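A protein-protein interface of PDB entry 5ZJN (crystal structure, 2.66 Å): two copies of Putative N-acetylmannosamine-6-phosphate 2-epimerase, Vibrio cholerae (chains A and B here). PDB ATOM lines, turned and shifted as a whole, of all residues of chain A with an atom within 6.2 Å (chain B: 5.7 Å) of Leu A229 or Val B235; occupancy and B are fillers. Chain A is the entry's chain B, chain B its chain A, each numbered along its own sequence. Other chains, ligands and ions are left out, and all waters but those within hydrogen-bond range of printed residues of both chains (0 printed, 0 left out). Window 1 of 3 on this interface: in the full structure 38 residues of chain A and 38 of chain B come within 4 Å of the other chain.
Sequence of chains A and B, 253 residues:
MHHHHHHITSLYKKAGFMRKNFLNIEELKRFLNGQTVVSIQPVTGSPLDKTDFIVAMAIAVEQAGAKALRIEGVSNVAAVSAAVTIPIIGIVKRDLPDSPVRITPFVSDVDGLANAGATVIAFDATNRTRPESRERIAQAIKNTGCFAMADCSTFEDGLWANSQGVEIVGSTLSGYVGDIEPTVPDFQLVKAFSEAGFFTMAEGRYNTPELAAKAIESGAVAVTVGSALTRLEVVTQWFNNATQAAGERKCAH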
ATOM      1  N   THR A  36      19.232  20.856  20.138  1.00  0.00           N
ATOM      2  CA  THR A  36      18.409  21.780  19.359  1.00  0.00           C
ATOM      3  C   THR A  36      18.577  23.179  19.942  1.00  0.00           C
ATOM      4  O   THR A  36      18.282  23.405  21.117  1.00  0.00           O
ATOM      5  CB  THR A  36      16.928  21.361  19.376  1.00  0.00           C
ATOM      6  OG1 THR A  36      16.771  20.043  18.831  1.00  0.00           O
ATOM      7  CG2 THR A  36      16.066  22.337  18.586  1.00  0.00           C
ATOM      8  N   VAL A  37      19.057  24.107  19.131  1.00  0.00           N
ATOM      9  CA  VAL A  37      19.218  25.491  19.560  1.00  0.00           C
ATOM     10  C   VAL A  37      17.970  26.261  19.155  1.00  0.00           C
ATOM     11  O   VAL A  37      17.596  26.292  17.976  1.00  0.00           O
ATOM     12  CB  VAL A  37      20.498  26.124  18.963  1.00  0.00           C
ATOM     13  CG1 VAL A  37      20.752  27.523  19.539  1.00  0.00           C
ATOM     14  CG2 VAL A  37      21.720  25.240  19.232  1.00  0.00           C
ATOM     15  N   VAL A  38      17.340  26.900  20.131  1.00  0.00           N
ATOM     16  CA  VAL A  38      16.062  27.565  19.938  1.00  0.00           C
ATOM     17  C   VAL A  38      16.358  29.020  19.589  1.00  0.00           C
ATOM     18  O   VAL A  38      16.836  29.777  20.432  1.00  0.00           O
ATOM     19  CB  VAL A  38      15.192  27.473  21.202  1.00  0.00           C
ATOM     20  CG1 VAL A  38      13.899  28.272  21.043  1.00  0.00           C
ATOM     21  CG2 VAL A  38      14.909  26.025  21.586  1.00  0.00           C
ATOM     22  N   SER A  39      16.027  29.428  18.366  1.00  0.00           N
ATOM     23  CA  SER A  39      16.179  30.816  17.956  1.00  0.00           C
ATOM     24  C   SER A  39      14.899  31.552  18.305  1.00  0.00           C
ATOM     25  O   SER A  39      13.883  31.398  17.626  1.00  0.00           O
ATOM     26  CB  SER A  39      16.479  30.923  16.463  1.00  0.00           C
ATOM     27  OG  SER A  39      16.639  32.274  16.064  1.00  0.00           O
ATOM     28  N   MET A  57       9.995  33.320  27.105  1.00  0.00           N
ATOM     29  CA  MET A  57      10.265  32.152  26.276  1.00  0.00           C
ATOM     30  C   MET A  57      11.651  31.585  26.553  1.00  0.00           C
ATOM     31  O   MET A  57      11.832  30.362  26.586  1.00  0.00           O
ATOM     32  CB  MET A  57      10.124  32.508  24.796  1.00  0.00           C
ATOM     33  CG  MET A  57       8.728  32.816  24.336  1.00  0.00           C
ATOM     34  SD  MET A  57       8.536  33.060  22.539  1.00  0.00           S
ATOM     35  CE  MET A  57       8.840  34.805  22.363  1.00  0.00           C
ATOM     36  N   PRO A 209      10.790  17.910  13.848  1.00  0.00           N
ATOM     37  CA  PRO A 209      11.866  17.200  14.579  1.00  0.00           C
ATOM     38  C   PRO A 209      12.585  16.163  13.741  1.00  0.00           C
ATOM     39  O   PRO A 209      13.703  15.763  14.093  1.00  0.00           O
ATOM     40  CB  PRO A 209      11.127  16.557  15.764  1.00  0.00           C
ATOM     41  CG  PRO A 209       9.893  17.429  15.951  1.00  0.00           C
ATOM     42  CD  PRO A 209       9.510  17.908  14.584  1.00  0.00           C
ATOM     43  N   VAL A 225      16.561  26.092  15.407  1.00  0.00           N
ATOM     44  CA  VAL A 225      15.180  26.074  14.956  1.00  0.00           C
ATOM     45  C   VAL A 225      14.504  27.344  15.450  1.00  0.00           C
ATOM     46  O   VAL A 225      14.482  27.612  16.658  1.00  0.00           O
ATOM     47  CB  VAL A 225      14.440  24.809  15.447  1.00  0.00           C
ATOM     48  CG1 VAL A 225      12.970  24.833  15.040  1.00  0.00           C
ATOM     49  CG2 VAL A 225      15.117  23.558  14.897  1.00  0.00           C
ATOM     50  N   GLY A 226      13.903  28.089  14.524  1.00  0.00           N
ATOM     51  CA  GLY A 226      13.294  29.350  14.879  1.00  0.00           C
ATOM     52  C   GLY A 226      11.817  29.463  14.575  1.00  0.00           C
ATOM     53  O   GLY A 226      11.000  29.476  15.498  1.00  0.00           O
ATOM     54  N   SER A 227      11.459  29.548  13.295  1.00  0.00           N
ATOM     55  CA  SER A 227      10.067  29.802  12.927  1.00  0.00           C
ATOM     56  C   SER A 227       9.115  28.760  13.526  1.00  0.00           C
ATOM     57  O   SER A 227       8.095  29.114  14.125  1.00  0.00           O
ATOM     58  CB  SER A 227       9.938  29.859  11.405  1.00  0.00           C
ATOM     59  OG  SER A 227      10.726  30.908  10.880  1.00  0.00           O
ATOM     60  N   ALA A 228       9.453  27.473  13.409  1.00  0.00           N
ATOM     61  CA  ALA A 228       8.577  26.411  13.903  1.00  0.00           C
ATOM     62  C   ALA A 228       8.380  26.434  15.412  1.00  0.00           C
ATOM     63  O   ALA A 228       7.548  25.674  15.913  1.00  0.00           O
ATOM     64  CB  ALA A 228       9.107  25.036  13.498  1.00  0.00           C
ATOM     65  N   LEU A 229       9.129  27.252  16.153  1.00  0.00           N
ATOM     66  CA  LEU A 229       9.012  27.277  17.608  1.00  0.00           C
ATOM     67  C   LEU A 229       8.557  28.611  18.180  1.00  0.00           C
ATOM     68  O   LEU A 229       7.744  28.619  19.106  1.00  0.00           O
ATOM     69  CB  LEU A 229      10.341  26.897  18.251  1.00  0.00           C
ATOM     70  CG  LEU A 229      10.751  25.433  18.261  1.00  0.00           C
ATOM     71  CD1 LEU A 229      12.198  25.316  18.743  1.00  0.00           C
ATOM     72  CD2 LEU A 229       9.804  24.596  19.140  1.00  0.00           C
ATOM     73  N   THR A 230       9.057  29.741  17.660  1.00  0.00           N
ATOM     74  CA  THR A 230       8.894  31.053  18.293  1.00  0.00           C
ATOM     75  C   THR A 230       8.293  32.104  17.355  1.00  0.00           C
ATOM     76  O   THR A 230       8.419  33.306  17.622  1.00  0.00           O
ATOM     77  CB  THR A 230      10.248  31.575  18.843  1.00  0.00           C
ATOM     78  OG1 THR A 230      11.166  31.835  17.767  1.00  0.00           O
ATOM     79  CG2 THR A 230      10.905  30.597  19.833  1.00  0.00           C
ATOM     80  N   ARG A 231       7.652  31.691  16.260  1.00  0.00           N
ATOM     81  CA  ARG A 231       6.940  32.594  15.340  1.00  0.00           C
ATOM     82  C   ARG A 231       5.500  32.094  15.182  1.00  0.00           C
ATOM     83  O   ARG A 231       5.164  31.367  14.239  1.00  0.00           O
ATOM     84  CB  ARG A 231       7.681  32.706  13.962  1.00  0.00           C
ATOM     85  CG  ARG A 231       8.862  33.642  13.969  1.00  0.00           C
ATOM     86  CD  ARG A 231       9.634  33.639  12.636  1.00  0.00           C
ATOM     87  NE  ARG A 231      10.650  34.691  12.631  1.00  0.00           N
ATOM     88  CZ  ARG A 231      11.812  34.618  11.990  1.00  0.00           C
ATOM     89  NH1 ARG A 231      12.146  33.525  11.321  1.00  0.00           N
ATOM     90  NH2 ARG A 231      12.655  35.627  12.047  1.00  0.00           N
ATOM     91  N   LEU A 232       4.645  32.508  16.117  1.00  0.00           N
ATOM     92  CA  LEU A 232       3.290  31.968  16.171  1.00  0.00           C
ATOM     93  C   LEU A 232       2.497  32.290  14.902  1.00  0.00           C
ATOM     94  O   LEU A 232       1.761  31.433  14.395  1.00  0.00           O
ATOM     95  CB  LEU A 232       2.583  32.486  17.424  1.00  0.00           C
ATOM     96  CG  LEU A 232       1.222  31.852  17.736  1.00  0.00           C
ATOM     97  CD1 LEU A 232       1.327  30.330  17.827  1.00  0.00           C
ATOM     98  CD2 LEU A 232       0.651  32.423  19.027  1.00  0.00           C
ATOM     99  N   VAL A 235       3.550  29.818  12.010  1.00  0.00           N
ATOM    100  CA  VAL A 235       3.064  28.448  12.161  1.00  0.00           C
ATOM    101  C   VAL A 235       1.543  28.397  12.014  1.00  0.00           C
ATOM    102  O   VAL A 235       1.006  27.481  11.384  1.00  0.00           O
ATOM    103  CB  VAL A 235       3.524  27.836  13.501  1.00  0.00           C
ATOM    104  CG1 VAL A 235       3.182  26.341  13.553  1.00  0.00           C
ATOM    105  CG2 VAL A 235       5.013  28.031  13.704  1.00  0.00           C
ATOM    106  N   SER B 227      -1.123  22.242  21.406  1.00  0.00           N
ATOM    107  CA  SER B 227       0.254  21.996  21.826  1.00  0.00           C
ATOM    108  C   SER B 227       1.252  22.416  20.756  1.00  0.00           C
ATOM    109  O   SER B 227       2.234  23.106  21.050  1.00  0.00           O
ATOM    110  CB  SER B 227       0.433  20.516  22.175  1.00  0.00           C
ATOM    111  OG  SER B 227      -0.454  20.145  23.209  1.00  0.00           O
ATOM    112  N   ALA B 228       1.013  22.024  19.509  1.00  0.00           N
ATOM    113  CA  ALA B 228       1.934  22.351  18.433  1.00  0.00           C
ATOM    114  C   ALA B 228       2.038  23.857  18.162  1.00  0.00           C
ATOM    115  O   ALA B 228       2.913  24.273  17.395  1.00  0.00           O
ATOM    116  CB  ALA B 228       1.526  21.591  17.168  1.00  0.00           C
ATOM    117  N   LEU B 229       1.181  24.675  18.765  1.00  0.00           N
ATOM    118  CA  LEU B 229       1.156  26.118  18.545  1.00  0.00           C
ATOM    119  C   LEU B 229       1.412  26.957  19.788  1.00  0.00           C
ATOM    120  O   LEU B 229       2.115  27.964  19.693  1.00  0.00           O
ATOM    121  CB  LEU B 229      -0.199  26.534  17.931  1.00  0.00           C
ATOM    122  CG  LEU B 229      -0.387  26.275  16.447  1.00  0.00           C
ATOM    123  CD1 LEU B 229      -1.852  26.491  16.040  1.00  0.00           C
ATOM    124  CD2 LEU B 229       0.517  27.209  15.689  1.00  0.00           C
ATOM    125  N   ARG B 231       2.229  25.738  23.176  1.00  0.00           N
ATOM    126  CA  ARG B 231       2.948  25.102  24.273  1.00  0.00           C
ATOM    127  C   ARG B 231       4.411  24.946  23.855  1.00  0.00           C
ATOM    128  O   ARG B 231       4.817  23.898  23.345  1.00  0.00           O
ATOM    129  CB  ARG B 231       2.285  23.762  24.650  1.00  0.00           C
ATOM    130  CG  ARG B 231       1.043  23.935  25.486  1.00  0.00           C
ATOM    131  CD  ARG B 231       0.379  22.617  25.799  1.00  0.00           C
ATOM    132  NE  ARG B 231      -0.714  22.809  26.752  1.00  0.00           N
ATOM    133  CZ  ARG B 231      -1.790  22.029  26.832  1.00  0.00           C
ATOM    134  NH1 ARG B 231      -1.940  21.017  25.993  1.00  0.00           N
ATOM    135  NH2 ARG B 231      -2.732  22.294  27.724  1.00  0.00           N
ATOM    136  N   LEU B 232       5.194  26.014  24.063  1.00  0.00           N
ATOM    137  CA  LEU B 232       6.585  26.037  23.611  1.00  0.00           C
ATOM    138  C   LEU B 232       7.411  24.939  24.282  1.00  0.00           C
ATOM    139  O   LEU B 232       8.208  24.262  23.621  1.00  0.00           O
ATOM    140  CB  LEU B 232       7.186  27.421  23.886  1.00  0.00           C
ATOM    141  CG  LEU B 232       8.615  27.823  23.446  1.00  0.00           C
ATOM    142  CD1 LEU B 232       8.860  27.663  21.947  1.00  0.00           C
ATOM    143  CD2 LEU B 232       8.972  29.234  23.910  1.00  0.00           C
ATOM    144  N   GLU B 233       7.207  24.722  25.587  1.00  0.00           N
ATOM    145  CA  GLU B 233       7.959  23.682  26.297  1.00  0.00           C
ATOM    146  C   GLU B 233       7.782  22.321  25.637  1.00  0.00           C
ATOM    147  O   GLU B 233       8.753  21.575  25.453  1.00  0.00           O
ATOM    148  CB  GLU B 233       7.479  23.601  27.747  1.00  0.00           C
ATOM    149  CG  GLU B 233       7.812  24.804  28.628  1.00  0.00           C
ATOM    150  CD  GLU B 233       6.747  25.890  28.541  1.00  0.00           C
ATOM    151  OE1 GLU B 233       6.102  25.998  27.471  1.00  0.00           O
ATOM    152  OE2 GLU B 233       6.542  26.613  29.540  1.00  0.00           O
ATOM    153  N   VAL B 234       6.538  22.004  25.252  1.00  0.00           N
ATOM    154  CA  VAL B 234       6.196  20.735  24.619  1.00  0.00           C
ATOM    155  C   VAL B 234       6.865  20.601  23.255  1.00  0.00           C
ATOM    156  O   VAL B 234       7.482  19.570  22.952  1.00  0.00           O
ATOM    157  CB  VAL B 234       4.667  20.601  24.516  1.00  0.00           C
ATOM    158  CG1 VAL B 234       4.286  19.446  23.597  1.00  0.00           C
ATOM    159  CG2 VAL B 234       4.055  20.419  25.892  1.00  0.00           C
ATOM    160  N   VAL B 235       6.716  21.619  22.391  1.00  0.00           N
ATOM    161  CA  VAL B 235       7.273  21.518  21.041  1.00  0.00           C
ATOM    162  C   VAL B 235       8.790  21.468  21.110  1.00  0.00           C
ATOM    163  O   VAL B 235       9.439  20.756  20.332  1.00  0.00           O
ATOM    164  CB  VAL B 235       6.792  22.673  20.137  1.00  0.00           C
ATOM    165  CG1 VAL B 235       7.102  22.350  18.705  1.00  0.00           C
ATOM    166  CG2 VAL B 235       5.312  22.981  20.309  1.00  0.00           C
ATOM    167  N   THR B 236       9.377  22.217  22.055  1.00  0.00           N
ATOM    168  CA  THR B 236      10.818  22.153  22.295  1.00  0.00           C
ATOM    169  C   THR B 236      11.270  20.732  22.617  1.00  0.00           C
ATOM    170  O   THR B 236      12.246  20.236  22.039  1.00  0.00           O
ATOM    171  CB  THR B 236      11.211  23.114  23.424  1.00  0.00           C
ATOM    172  OG1 THR B 236      11.128  24.473  22.973  1.00  0.00           O
ATOM    173  CG2 THR B 236      12.617  22.825  23.920  1.00  0.00           C
ATOM    174  N   GLN B 237      10.571  20.057  23.541  1.00  0.00           N
ATOM    175  CA  GLN B 237      10.944  18.685  23.905  1.00  0.00           C
ATOM    176  C   GLN B 237      10.697  17.700  22.769  1.00  0.00           C
ATOM    177  O   GLN B 237      11.344  16.652  22.713  1.00  0.00           O
ATOM    178  CB  GLN B 237      10.193  18.251  25.164  1.00  0.00           C
ATOM    179  CG  GLN B 237      10.636  18.973  26.432  1.00  0.00           C
ATOM    180  CD  GLN B 237       9.774  18.629  27.629  1.00  0.00           C
ATOM    181  OE1 GLN B 237       8.625  18.222  27.474  1.00  0.00           O
ATOM    182  NE2 GLN B 237      10.325  18.780  28.826  1.00  0.00           N
ATOM    183  N   TRP B 238       9.785  18.019  21.850  1.00  0.00           N
ATOM    184  CA  TRP B 238       9.642  17.203  20.647  1.00  0.00           C
ATOM    185  C   TRP B 238      10.906  17.243  19.802  1.00  0.00           C
ATOM    186  O   TRP B 238      11.322  16.222  19.239  1.00  0.00           O
ATOM    187  CB  TRP B 238       8.451  17.683  19.819  1.00  0.00           C
ATOM    188  CG  TRP B 238       7.115  17.329  20.384  1.00  0.00           C
ATOM    189  CD1 TRP B 238       6.849  16.437  21.395  1.00  0.00           C
ATOM    190  CD2 TRP B 238       5.848  17.860  19.971  1.00  0.00           C
ATOM    191  NE1 TRP B 238       5.498  16.389  21.631  1.00  0.00           N
ATOM    192  CE2 TRP B 238       4.859  17.243  20.770  1.00  0.00           C
ATOM    193  CE3 TRP B 238       5.455  18.790  19.000  1.00  0.00           C
ATOM    194  CZ2 TRP B 238       3.501  17.529  20.632  1.00  0.00           C
ATOM    195  CZ3 TRP B 238       4.114  19.079  18.868  1.00  0.00           C
ATOM    196  CH2 TRP B 238       3.146  18.444  19.682  1.00  0.00           C
ATOM    197  N   PHE B 239      11.523  18.425  19.692  1.00  0.00           N
ATOM    198  CA  PHE B 239      12.708  18.576  18.855  1.00  0.00           C
ATOM    199  C   PHE B 239      13.945  17.961  19.507  1.00  0.00           C
ATOM    200  O   PHE B 239      14.683  17.207  18.861  1.00  0.00           O
ATOM    201  CB  PHE B 239      12.931  20.047  18.528  1.00  0.00           C
ATOM    202  CG  PHE B 239      12.075  20.562  17.407  1.00  0.00           C
ATOM    203  CD1 PHE B 239      12.461  20.382  16.088  1.00  0.00           C
ATOM    204  CD2 PHE B 239      10.908  21.266  17.664  1.00  0.00           C
ATOM    205  CE1 PHE B 239      11.690  20.872  15.051  1.00  0.00           C
ATOM    206  CE2 PHE B 239      10.135  21.758  16.625  1.00  0.00           C
ATOM    207  CZ  PHE B 239      10.525  21.558  15.319  1.00  0.00           C
ATOM    208  N   ASN B 240      14.198  18.278  20.782  1.00  0.00           N
ATOM    209  CA  ASN B 240      15.411  17.768  21.429  1.00  0.00           C
ATOM    210  C   ASN B 240      15.424  16.245  21.493  1.00  0.00           C
ATOM    211  O   ASN B 240      16.477  15.623  21.317  1.00  0.00           O
ATOM    212  CB  ASN B 240      15.573  18.356  22.831  1.00  0.00           C
ATOM    213  CG  ASN B 240      16.502  19.557  22.856  1.00  0.00           C
ATOM    214  OD1 ASN B 240      17.307  19.748  21.944  1.00  0.00           O
ATOM    215  ND2 ASN B 240      16.406  20.369  23.914  1.00  0.00           N
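Among the printed residues, pairs that only touch across the chains: Leu A232 with Leu B229, Leu A229 with Leu B232, Pro A209 with Phe B239, Pro A209 with Trp B238, Thr A36 with Phe B239, Val A235 with Leu B229, Leu A229 with Val B235, Met A57 with Leu B232, Leu A229 with Thr B236 and Leu A229 with Phe B239.
OD1 of Asn B240 sits at hydrogen-bond distance from N of Thr A36 (2.9 Å).
Leu A229 touches Leu B232, and with the chains exchanged Leu A232 touches Leu B229. Leu A229 touches Val B235, and with the chains exchanged Val A235 touches Leu B229. Positions printed for both chains: 227, 228, 229, 231, 232 and 235. Of the 11 pairs that touch across the chains among the printed residues, 4 have their exchanged pair printed and touching as well.
The backbone carbonyl oxygen (O) of Leu B232 is in hydrogen-bond range of the side-chain hydroxyl (OG1) of Thr B236 (3.0 Å).
Of the 13 printed residues of chain B, 7 touch a printed residue of chain A. Hydrophobic or aromatic side chains of chain B within 4 Å of the printed part of chain A: Leu B229, Leu B232, Val B235 and Phe B239. Hydrophobic or aromatic side chains of chain A that line the printed part of chain B: Met A57, Pro A209, Leu A229, Leu A232 and Val A235. Among the printed residues, 11 pairs touch across the chains.
Val B235 touches one residue of chain A. Of the printed residues of chain B, Pro A209 touches Trp B238 (3.5 Å) and Phe B239 (3.3 Å). Of the printed residues of chain A, Phe B239 touches Thr A36, Pro A209 and Leu A229. Of the printed residues of chain A, Leu B229 touches Leu A232 and Val A235. Printed residues of chain B within 4 Å of Val A235: Leu B229 (3.5 Å). Printed residues of chain A within 4 Å of Trp B238: Pro A209. The nearest printed residue of chain B that does not touch Leu A229 is Leu B229 (5.7 Å). The nearest residue of chain A that does not touch Val B235 is Ala A228 (4.4 Å).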
